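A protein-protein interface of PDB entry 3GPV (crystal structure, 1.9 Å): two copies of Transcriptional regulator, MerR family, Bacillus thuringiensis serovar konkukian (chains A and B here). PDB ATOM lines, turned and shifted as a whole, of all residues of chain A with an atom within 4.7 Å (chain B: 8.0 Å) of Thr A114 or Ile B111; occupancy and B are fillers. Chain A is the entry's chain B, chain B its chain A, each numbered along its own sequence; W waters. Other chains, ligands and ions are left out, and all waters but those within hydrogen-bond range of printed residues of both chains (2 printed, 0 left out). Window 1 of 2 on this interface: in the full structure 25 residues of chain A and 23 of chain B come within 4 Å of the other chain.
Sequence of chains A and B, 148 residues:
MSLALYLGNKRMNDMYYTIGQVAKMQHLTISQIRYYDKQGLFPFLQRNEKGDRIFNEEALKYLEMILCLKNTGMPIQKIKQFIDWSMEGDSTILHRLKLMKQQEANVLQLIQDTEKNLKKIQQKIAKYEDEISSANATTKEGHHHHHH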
ATOM      1  N   LEU A 110     -17.443   6.784 -13.708  1.00  0.00           N
ATOM      2  CA  LEU A 110     -18.030   7.225 -14.960  1.00  0.00           C
ATOM      3  C   LEU A 110     -18.890   8.466 -14.752  1.00  0.00           C
ATOM      4  O   LEU A 110     -18.815   9.408 -15.531  1.00  0.00           O
ATOM      5  CB  LEU A 110     -18.866   6.100 -15.577  1.00  0.00           C
ATOM      6  CG  LEU A 110     -19.683   6.419 -16.840  1.00  0.00           C
ATOM      7  CD1 LEU A 110     -18.763   6.897 -17.962  1.00  0.00           C
ATOM      8  CD2 LEU A 110     -20.467   5.175 -17.269  1.00  0.00           C
ATOM      9  N   ILE A 111     -19.705   8.467 -13.702  1.00  0.00           N
ATOM     10  CA  ILE A 111     -20.566   9.616 -13.421  1.00  0.00           C
ATOM     11  C   ILE A 111     -19.681  10.829 -13.106  1.00  0.00           C
ATOM     12  O   ILE A 111     -19.902  11.925 -13.599  1.00  0.00           O
ATOM     13  CB  ILE A 111     -21.512   9.353 -12.195  1.00  0.00           C
ATOM     14  CG1 ILE A 111     -22.699   8.480 -12.604  1.00  0.00           C
ATOM     15  CG2 ILE A 111     -22.082  10.659 -11.674  1.00  0.00           C
ATOM     16  CD1 ILE A 111     -22.346   7.151 -13.058  1.00  0.00           C
ATOM     17  N   GLN A 112     -18.664  10.630 -12.284  1.00  0.00           N
ATOM     18  CA  GLN A 112     -17.801  11.752 -11.942  1.00  0.00           C
ATOM     19  C   GLN A 112     -17.089  12.290 -13.180  1.00  0.00           C
ATOM     20  O   GLN A 112     -17.014  13.501 -13.375  1.00  0.00           O
ATOM     21  CB  GLN A 112     -16.786  11.346 -10.881  1.00  0.00           C
ATOM     22  CG  GLN A 112     -15.810  12.467 -10.557  1.00  0.00           C
ATOM     23  CD  GLN A 112     -14.985  12.175  -9.332  1.00  0.00           C
ATOM     24  OE1 GLN A 112     -15.476  12.281  -8.205  1.00  0.00           O
ATOM     25  NE2 GLN A 112     -13.723  11.783  -9.539  1.00  0.00           N
ATOM     26  N   ASP A 113     -16.580  11.389 -14.015  1.00  0.00           N
ATOM     27  CA  ASP A 113     -15.907  11.801 -15.247  1.00  0.00           C
ATOM     28  C   ASP A 113     -16.864  12.558 -16.153  1.00  0.00           C
ATOM     29  O   ASP A 113     -16.468  13.514 -16.814  1.00  0.00           O
ATOM     30  CB  ASP A 113     -15.357  10.595 -15.997  1.00  0.00           C
ATOM     31  CG  ASP A 113     -14.172   9.970 -15.295  1.00  0.00           C
ATOM     32  OD1 ASP A 113     -13.589  10.633 -14.417  1.00  0.00           O
ATOM     33  OD2 ASP A 113     -13.826   8.825 -15.630  1.00  0.00           O
ATOM     34  N   THR A 114     -18.125  12.129 -16.173  1.00  0.00           N
ATOM     35  CA  THR A 114     -19.137  12.770 -17.022  1.00  0.00           C
ATOM     36  C   THR A 114     -19.508  14.138 -16.461  1.00  0.00           C
ATOM     37  O   THR A 114     -19.726  15.092 -17.209  1.00  0.00           O
ATOM     38  CB  THR A 114     -20.395  11.886 -17.170  1.00  0.00           C
ATOM     39  OG1 THR A 114     -20.018  10.606 -17.670  1.00  0.00           O
ATOM     40  CG2 THR A 114     -21.368  12.507 -18.167  1.00  0.00           C
ATOM     41  N   GLU A 115     -19.569  14.241 -15.138  1.00  0.00           N
ATOM     42  CA  GLU A 115     -19.860  15.532 -14.531  1.00  0.00           C
ATOM     43  C   GLU A 115     -18.715  16.494 -14.905  1.00  0.00           C
ATOM     44  O   GLU A 115     -18.938  17.678 -15.206  1.00  0.00           O
ATOM     45  CB  GLU A 115     -19.953  15.400 -13.005  1.00  0.00           C
ATOM     46  CG  GLU A 115     -21.178  14.660 -12.513  1.00  0.00           C
ATOM     47  CD  GLU A 115     -22.444  15.509 -12.536  1.00  0.00           C
ATOM     48  OE1 GLU A 115     -22.430  16.649 -13.045  1.00  0.00           O
ATOM     49  OE2 GLU A 115     -23.470  15.017 -12.037  1.00  0.00           O
ATOM     50  N   LYS A 116     -17.488  15.974 -14.900  1.00  0.00           N
ATOM     51  CA  LYS A 116     -16.331  16.802 -15.231  1.00  0.00           C
ATOM     52  C   LYS A 116     -16.425  17.293 -16.674  1.00  0.00           C
ATOM     53  O   LYS A 116     -16.101  18.448 -16.970  1.00  0.00           O
ATOM     54  CB  LYS A 116     -15.034  16.028 -15.019  1.00  0.00           C
ATOM     55  CG  LYS A 116     -13.817  16.772 -15.566  1.00  0.00           C
ATOM     56  CD  LYS A 116     -12.568  16.647 -14.706  1.00  0.00           C
ATOM     57  CE  LYS A 116     -12.292  15.214 -14.297  1.00  0.00           C
ATOM     58  NZ  LYS A 116     -13.143  14.795 -13.145  1.00  0.00           N
ATOM     59  N   ASN A 117     -16.879  16.416 -17.567  1.00  0.00           N
ATOM     60  CA  ASN A 117     -17.038  16.785 -18.962  1.00  0.00           C
ATOM     61  C   ASN A 117     -18.159  17.805 -19.112  1.00  0.00           C
ATOM     62  O   ASN A 117     -18.038  18.764 -19.877  1.00  0.00           O
ATOM     63  CB  ASN A 117     -17.287  15.535 -19.826  1.00  0.00           C
ATOM     64  CG  ASN A 117     -15.989  14.755 -20.076  1.00  0.00           C
ATOM     65  OD1 ASN A 117     -14.975  15.359 -20.364  1.00  0.00           O
ATOM     66  ND2 ASN A 117     -16.026  13.437 -19.961  1.00  0.00           N
ATOM     67  N   LEU A 118     -19.232  17.616 -18.347  1.00  0.00           N
ATOM     68  CA  LEU A 118     -20.369  18.536 -18.377  1.00  0.00           C
ATOM     69  C   LEU A 118     -19.883  19.952 -18.031  1.00  0.00           C
ATOM     70  O   LEU A 118     -20.345  20.935 -18.596  1.00  0.00           O
ATOM     71  CB  LEU A 118     -21.422  18.100 -17.354  1.00  0.00           C
ATOM     72  CG  LEU A 118     -22.654  19.008 -17.239  1.00  0.00           C
ATOM     73  CD1 LEU A 118     -23.372  19.134 -18.599  1.00  0.00           C
ATOM     74  CD2 LEU A 118     -23.606  18.431 -16.198  1.00  0.00           C
ATOM     75  N   CYS B  68     -13.275  15.737 -24.647  1.00  0.00           N
ATOM     76  CA  CYS B  68     -14.517  15.880 -23.906  1.00  0.00           C
ATOM     77  C   CYS B  68     -15.703  15.393 -24.752  1.00  0.00           C
ATOM     78  O   CYS B  68     -16.520  14.573 -24.319  1.00  0.00           O
ATOM     79  CB  CYS B  68     -14.728  17.345 -23.538  1.00  0.00           C
ATOM     80  SG  CYS B  68     -16.287  17.635 -22.678  1.00  0.00           S
ATOM     81  N   ASN B  71     -15.453  11.700 -25.406  1.00  0.00           N
ATOM     82  CA  ASN B  71     -15.795  10.950 -24.211  1.00  0.00           C
ATOM     83  C   ASN B  71     -17.248  11.102 -23.769  1.00  0.00           C
ATOM     84  O   ASN B  71     -17.671  10.471 -22.798  1.00  0.00           O
ATOM     85  CB  ASN B  71     -14.844  11.342 -23.079  1.00  0.00           C
ATOM     86  CG  ASN B  71     -13.409  10.902 -23.348  1.00  0.00           C
ATOM     87  OD1 ASN B  71     -12.467  11.416 -22.751  1.00  0.00           O
ATOM     88  ND2 ASN B  71     -13.244   9.938 -24.243  1.00  0.00           N
ATOM     89  N   THR B  72     -18.006  11.939 -24.469  1.00  0.00           N
ATOM     90  CA  THR B  72     -19.409  12.112 -24.142  1.00  0.00           C
ATOM     91  C   THR B  72     -20.273  11.639 -25.303  1.00  0.00           C
ATOM     92  O   THR B  72     -21.417  12.053 -25.443  1.00  0.00           O
ATOM     93  CB  THR B  72     -19.756  13.579 -23.760  1.00  0.00           C
ATOM     94  OG1 THR B  72     -19.252  14.486 -24.753  1.00  0.00           O
ATOM     95  CG2 THR B  72     -19.161  13.919 -22.417  1.00  0.00           C
ATOM     96  N   GLU B 104     -24.783  19.577 -23.952  1.00  0.00           N
ATOM     97  CA  GLU B 104     -25.069  19.705 -22.524  1.00  0.00           C
ATOM     98  C   GLU B 104     -26.348  18.887 -22.276  1.00  0.00           C
ATOM     99  O   GLU B 104     -26.454  18.077 -21.338  1.00  0.00           O
ATOM    100  CB  GLU B 104     -25.288  21.181 -22.158  1.00  0.00           C
ATOM    101  CG  GLU B 104     -25.744  21.392 -20.713  1.00  0.00           C
ATOM    102  CD  GLU B 104     -26.129  22.843 -20.362  1.00  0.00           C
ATOM    103  OE1 GLU B 104     -26.807  23.520 -21.171  1.00  0.00           O
ATOM    104  OE2 GLU B 104     -25.769  23.303 -19.256  1.00  0.00           O
ATOM    105  N   ALA B 105     -27.338  19.109 -23.131  1.00  0.00           N
ATOM    106  CA  ALA B 105     -28.579  18.364 -22.994  1.00  0.00           C
ATOM    107  C   ALA B 105     -28.280  16.856 -23.070  1.00  0.00           C
ATOM    108  O   ALA B 105     -28.777  16.069 -22.252  1.00  0.00           O
ATOM    109  CB  ALA B 105     -29.583  18.798 -24.099  1.00  0.00           C
ATOM    110  N   ASN B 106     -27.447  16.459 -24.031  1.00  0.00           N
ATOM    111  CA  ASN B 106     -27.080  15.056 -24.197  1.00  0.00           C
ATOM    112  C   ASN B 106     -26.333  14.513 -22.979  1.00  0.00           C
ATOM    113  O   ASN B 106     -26.538  13.375 -22.567  1.00  0.00           O
ATOM    114  CB  ASN B 106     -26.169  14.847 -25.426  1.00  0.00           C
ATOM    115  CG  ASN B 106     -26.915  14.930 -26.744  1.00  0.00           C
ATOM    116  OD1 ASN B 106     -28.081  14.560 -26.833  1.00  0.00           O
ATOM    117  ND2 ASN B 106     -26.231  15.395 -27.782  1.00  0.00           N
ATOM    118  N   VAL B 107     -25.464  15.325 -22.404  1.00  0.00           N
ATOM    119  CA  VAL B 107     -24.687  14.839 -21.283  1.00  0.00           C
ATOM    120  C   VAL B 107     -25.545  14.732 -20.017  1.00  0.00           C
ATOM    121  O   VAL B 107     -25.367  13.824 -19.220  1.00  0.00           O
ATOM    122  CB  VAL B 107     -23.419  15.710 -21.065  1.00  0.00           C
ATOM    123  CG1 VAL B 107     -22.654  15.213 -19.848  1.00  0.00           C
ATOM    124  CG2 VAL B 107     -22.501  15.613 -22.285  1.00  0.00           C
ATOM    125  N   LEU B 108     -26.494  15.648 -19.852  1.00  0.00           N
ATOM    126  CA  LEU B 108     -27.378  15.582 -18.707  1.00  0.00           C
ATOM    127  C   LEU B 108     -28.176  14.266 -18.812  1.00  0.00           C
ATOM    128  O   LEU B 108     -28.405  13.584 -17.821  1.00  0.00           O
ATOM    129  CB  LEU B 108     -28.310  16.800 -18.683  1.00  0.00           C
ATOM    130  CG  LEU B 108     -27.622  18.101 -18.235  1.00  0.00           C
ATOM    131  CD1 LEU B 108     -28.486  19.290 -18.560  1.00  0.00           C
ATOM    132  CD2 LEU B 108     -27.349  18.036 -16.737  1.00  0.00           C
ATOM    133  N   GLN B 109     -28.580  13.901 -20.024  1.00  0.00           N
ATOM    134  CA  GLN B 109     -29.313  12.645 -20.228  1.00  0.00           C
ATOM    135  C   GLN B 109     -28.400  11.429 -19.907  1.00  0.00           C
ATOM    136  O   GLN B 109     -28.842  10.431 -19.324  1.00  0.00           O
ATOM    137  CB  GLN B 109     -29.814  12.566 -21.674  1.00  0.00           C
ATOM    138  CG  GLN B 109     -30.648  11.333 -22.000  1.00  0.00           C
ATOM    139  CD  GLN B 109     -31.972  11.313 -21.262  1.00  0.00           C
ATOM    140  OE1 GLN B 109     -32.752  12.263 -21.333  1.00  0.00           O
ATOM    141  NE2 GLN B 109     -32.231  10.226 -20.544  1.00  0.00           N
ATOM    142  N   LEU B 110     -27.136  11.514 -20.295  1.00  0.00           N
ATOM    143  CA  LEU B 110     -26.184  10.440 -20.020  1.00  0.00           C
ATOM    144  C   LEU B 110     -26.107  10.213 -18.515  1.00  0.00           C
ATOM    145  O   LEU B 110     -26.194   9.084 -18.042  1.00  0.00           O
ATOM    146  CB  LEU B 110     -24.800  10.813 -20.537  1.00  0.00           C
ATOM    147  CG  LEU B 110     -24.282  10.097 -21.781  1.00  0.00           C
ATOM    148  CD1 LEU B 110     -22.964  10.720 -22.219  1.00  0.00           C
ATOM    149  CD2 LEU B 110     -24.105   8.619 -21.466  1.00  0.00           C
ATOM    150  N   ILE B 111     -25.936  11.302 -17.771  1.00  0.00           N
ATOM    151  CA  ILE B 111     -25.842  11.243 -16.317  1.00  0.00           C
ATOM    152  C   ILE B 111     -27.124  10.609 -15.770  1.00  0.00           C
ATOM    153  O   ILE B 111     -27.091   9.698 -14.947  1.00  0.00           O
ATOM    154  CB  ILE B 111     -25.721  12.639 -15.711  1.00  0.00           C
ATOM    155  CG1 ILE B 111     -24.386  13.289 -16.126  1.00  0.00           C
ATOM    156  CG2 ILE B 111     -25.850  12.549 -14.202  1.00  0.00           C
ATOM    157  CD1 ILE B 111     -23.164  12.539 -15.639  1.00  0.00           C
ATOM    158  N   GLN B 112     -28.261  11.113 -16.225  1.00  0.00           N
ATOM    159  CA  GLN B 112     -29.533  10.571 -15.769  1.00  0.00           C
ATOM    160  C   GLN B 112     -29.621   9.062 -16.021  1.00  0.00           C
ATOM    161  O   GLN B 112     -30.008   8.291 -15.140  1.00  0.00           O
ATOM    162  CB  GLN B 112     -30.693  11.268 -16.490  1.00  0.00           C
ATOM    163  CG  GLN B 112     -32.064  10.906 -15.931  1.00  0.00           C
ATOM    164  CD  GLN B 112     -33.194  11.396 -16.811  1.00  0.00           C
ATOM    165  OE1 GLN B 112     -33.248  12.567 -17.175  1.00  0.00           O
ATOM    166  NE2 GLN B 112     -34.102  10.495 -17.158  1.00  0.00           N
ATOM    167  N   ASP B 113     -29.256   8.647 -17.227  1.00  0.00           N
ATOM    168  CA  ASP B 113     -29.333   7.243 -17.584  1.00  0.00           C
ATOM    169  C   ASP B 113     -28.297   6.420 -16.841  1.00  0.00           C
ATOM    170  O   ASP B 113     -28.556   5.282 -16.450  1.00  0.00           O
ATOM    171  CB  ASP B 113     -29.166   7.058 -19.089  1.00  0.00           C
ATOM    172  CG  ASP B 113     -30.328   7.636 -19.883  1.00  0.00           C
ATOM    173  OD1 ASP B 113     -31.446   7.695 -19.336  1.00  0.00           O
ATOM    174  OD2 ASP B 113     -30.124   8.015 -21.050  1.00  0.00           O
ATOM    175  N   THR B 114     -27.124   6.998 -16.629  1.00  0.00           N
ATOM    176  CA  THR B 114     -26.089   6.254 -15.922  1.00  0.00           C
ATOM    177  C   THR B 114     -26.489   6.076 -14.463  1.00  0.00           C
ATOM    178  O   THR B 114     -26.199   5.049 -13.864  1.00  0.00           O
ATOM    179  CB  THR B 114     -24.726   6.944 -16.022  1.00  0.00           C
ATOM    180  OG1 THR B 114     -24.423   7.191 -17.393  1.00  0.00           O
ATOM    181  CG2 THR B 114     -23.642   6.032 -15.465  1.00  0.00           C
ATOM    182  N   GLU B 115     -27.174   7.064 -13.894  1.00  0.00           N
ATOM    183  CA  GLU B 115     -27.627   6.943 -12.503  1.00  0.00           C
ATOM    184  C   GLU B 115     -28.657   5.806 -12.409  1.00  0.00           C
ATOM    185  O   GLU B 115     -28.673   5.036 -11.452  1.00  0.00           O
ATOM    186  CB  GLU B 115     -28.266   8.240 -12.005  1.00  0.00           C
ATOM    187  CG  GLU B 115     -27.350   9.432 -11.973  1.00  0.00           C
ATOM    188  CD  GLU B 115     -28.078  10.698 -11.561  1.00  0.00           C
ATOM    189  OE1 GLU B 115     -29.215  10.908 -12.033  1.00  0.00           O
ATOM    190  OE2 GLU B 115     -27.512  11.489 -10.776  1.00  0.00           O
ATOM    191  N   LYS B 116     -29.522   5.723 -13.411  1.00  0.00           N
ATOM    192  CA  LYS B 116     -30.539   4.677 -13.467  1.00  0.00           C
ATOM    193  C   LYS B 116     -29.859   3.301 -13.494  1.00  0.00           C
ATOM    194  O   LYS B 116     -30.297   2.363 -12.836  1.00  0.00           O
ATOM    195  CB  LYS B 116     -31.406   4.863 -14.712  1.00  0.00           C
ATOM    196  CG  LYS B 116     -32.497   3.807 -14.892  1.00  0.00           C
ATOM    197  CD  LYS B 116     -33.447   3.767 -13.704  1.00  0.00           C
ATOM    198  CE  LYS B 116     -34.580   2.761 -13.927  1.00  0.00           C
ATOM    199  NZ  LYS B 116     -35.462   2.642 -12.727  1.00  0.00           N
ATOM    200  N   ASN B 117     -28.781   3.196 -14.257  1.00  0.00           N
ATOM    201  CA  ASN B 117     -28.048   1.953 -14.352  1.00  0.00           C
ATOM    202  C   ASN B 117     -27.313   1.658 -13.062  1.00  0.00           C
ATOM    203  O   ASN B 117     -27.209   0.504 -12.664  1.00  0.00           O
ATOM    204  CB  ASN B 117     -27.071   2.002 -15.526  1.00  0.00           C
ATOM    205  CG  ASN B 117     -27.788   2.037 -16.871  1.00  0.00           C
ATOM    206  OD1 ASN B 117     -28.825   1.402 -17.047  1.00  0.00           O
ATOM    207  ND2 ASN B 117     -27.229   2.775 -17.825  1.00  0.00           N
ATOM    208  N   LEU B 118     -26.804   2.700 -12.405  1.00  0.00           N
ATOM    209  CA  LEU B 118     -26.094   2.509 -11.147  1.00  0.00           C
ATOM    210  C   LEU B 118     -27.054   1.888 -10.129  1.00  0.00           C
ATOM    211  O   LEU B 118     -26.676   0.996  -9.378  1.00  0.00           O
ATOM    212  CB  LEU B 118     -25.569   3.841 -10.612  1.00  0.00           C
ATOM    213  CG  LEU B 118     -24.908   3.789  -9.223  1.00  0.00           C
ATOM    214  CD1 LEU B 118     -23.720   2.851  -9.261  1.00  0.00           C
ATOM    215  CD2 LEU B 118     -24.477   5.185  -8.800  1.00  0.00           C
HETATM  216  O   HOH W   1     -12.680  14.286 -21.423  1.00  0.00           O
HETATM  217  O   HOH W   2     -18.209  11.220 -20.023  1.00  0.00           O
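Water W1 bridges the side-chain amide oxygen of Asn A117 and the side-chain amide oxygen of Asn B71.
Water W2 lies within hydrogen-bond range of the backbone carbonyl oxygen (O) of Asn B71, the side-chain hydroxyl (OG1) of Thr A114 and the side-chain amide nitrogen (ND2) of Asn A117.
Of the printed residues of chain B, Ile A111 touches Ile B111 (3.9 Å) and Thr B114 (3.0 Å).
Of chain B, only Val B107 and Ile B111 come within 4 Å of Thr A114.
Of the printed residues of chain B, Leu A118 touches Glu B104 (3.9 Å) and Leu B108 (3.8 Å).
Printed residues of chain A within 4 Å of Cys B68: Asn A117 (3.5 Å).
Printed residues of chain A within 4 Å of Asn B71: Asn A117.
Printed residues of chain A within 4 Å of Val B107: Thr A114.
Of the printed residues of chain A, Ile B111 touches Ile A111 (3.9 Å) and Thr A114 (3.1 Å).
Leu B118 touches none of the printed residues of chain A.
The nearest residue of chain B that does not touch Thr A114 is Leu B110 (4.5 Å).
The nearest printed residue of chain A that does not touch Cys B68 is Leu A118 (5.2 Å).
O of Leu A110 lies within hydrogen-bond range of OG1 of Thr A114.
The backbone carbonyl oxygen (O) of Leu B110 sits at hydrogen-bond distance from the side-chain hydroxyl (OG1) of Thr B114, 2.7 Å away.
OG1 of Thr B72 is in hydrogen-bond range of O of Cys B68, at 2.8 Å.
O of Asp A113 sits at hydrogen-bond distance from ND2 of Asn A117 (3.2 Å).
Leu A110 touches Thr B114.
Ile A111 touches Ile B111 (O to CD1, 3.9 Å).
Ile A111 touches Thr B114 (CD1 to CG2, 3.0 Å).
CG2 of Thr A114 touches CG1 of Val B107, 3.4 Å away.
Thr A114 touches Ile B111.
ND2 of Asn A117 touches CB of Asn B71, at 3.9 Å.
CB of Asn A117 touches CG2 of Thr B72, 3.6 Å away.
Leu A118 touches Glu B104 (CD1 to CG, 3.9 Å).
Leu A118 touches Leu B108 (CD2 to CD2, 3.8 Å).
Leu A110 touches Thr B114, but with the chains exchanged Thr A114 does not touch Leu B110 (4.5 Å).
Ile A111 touches its own counterpart, Ile B111.
Ile A111 touches Thr B114, and with the chains exchanged Thr A114 touches Ile B111.
Of the 10 pairs that touch across the chains among the printed residues, 3 have their exchanged pair printed and touching as well.
SG of Cys B68 sits at hydrogen-bond distance from O of Asn A117 (3.5 Å).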
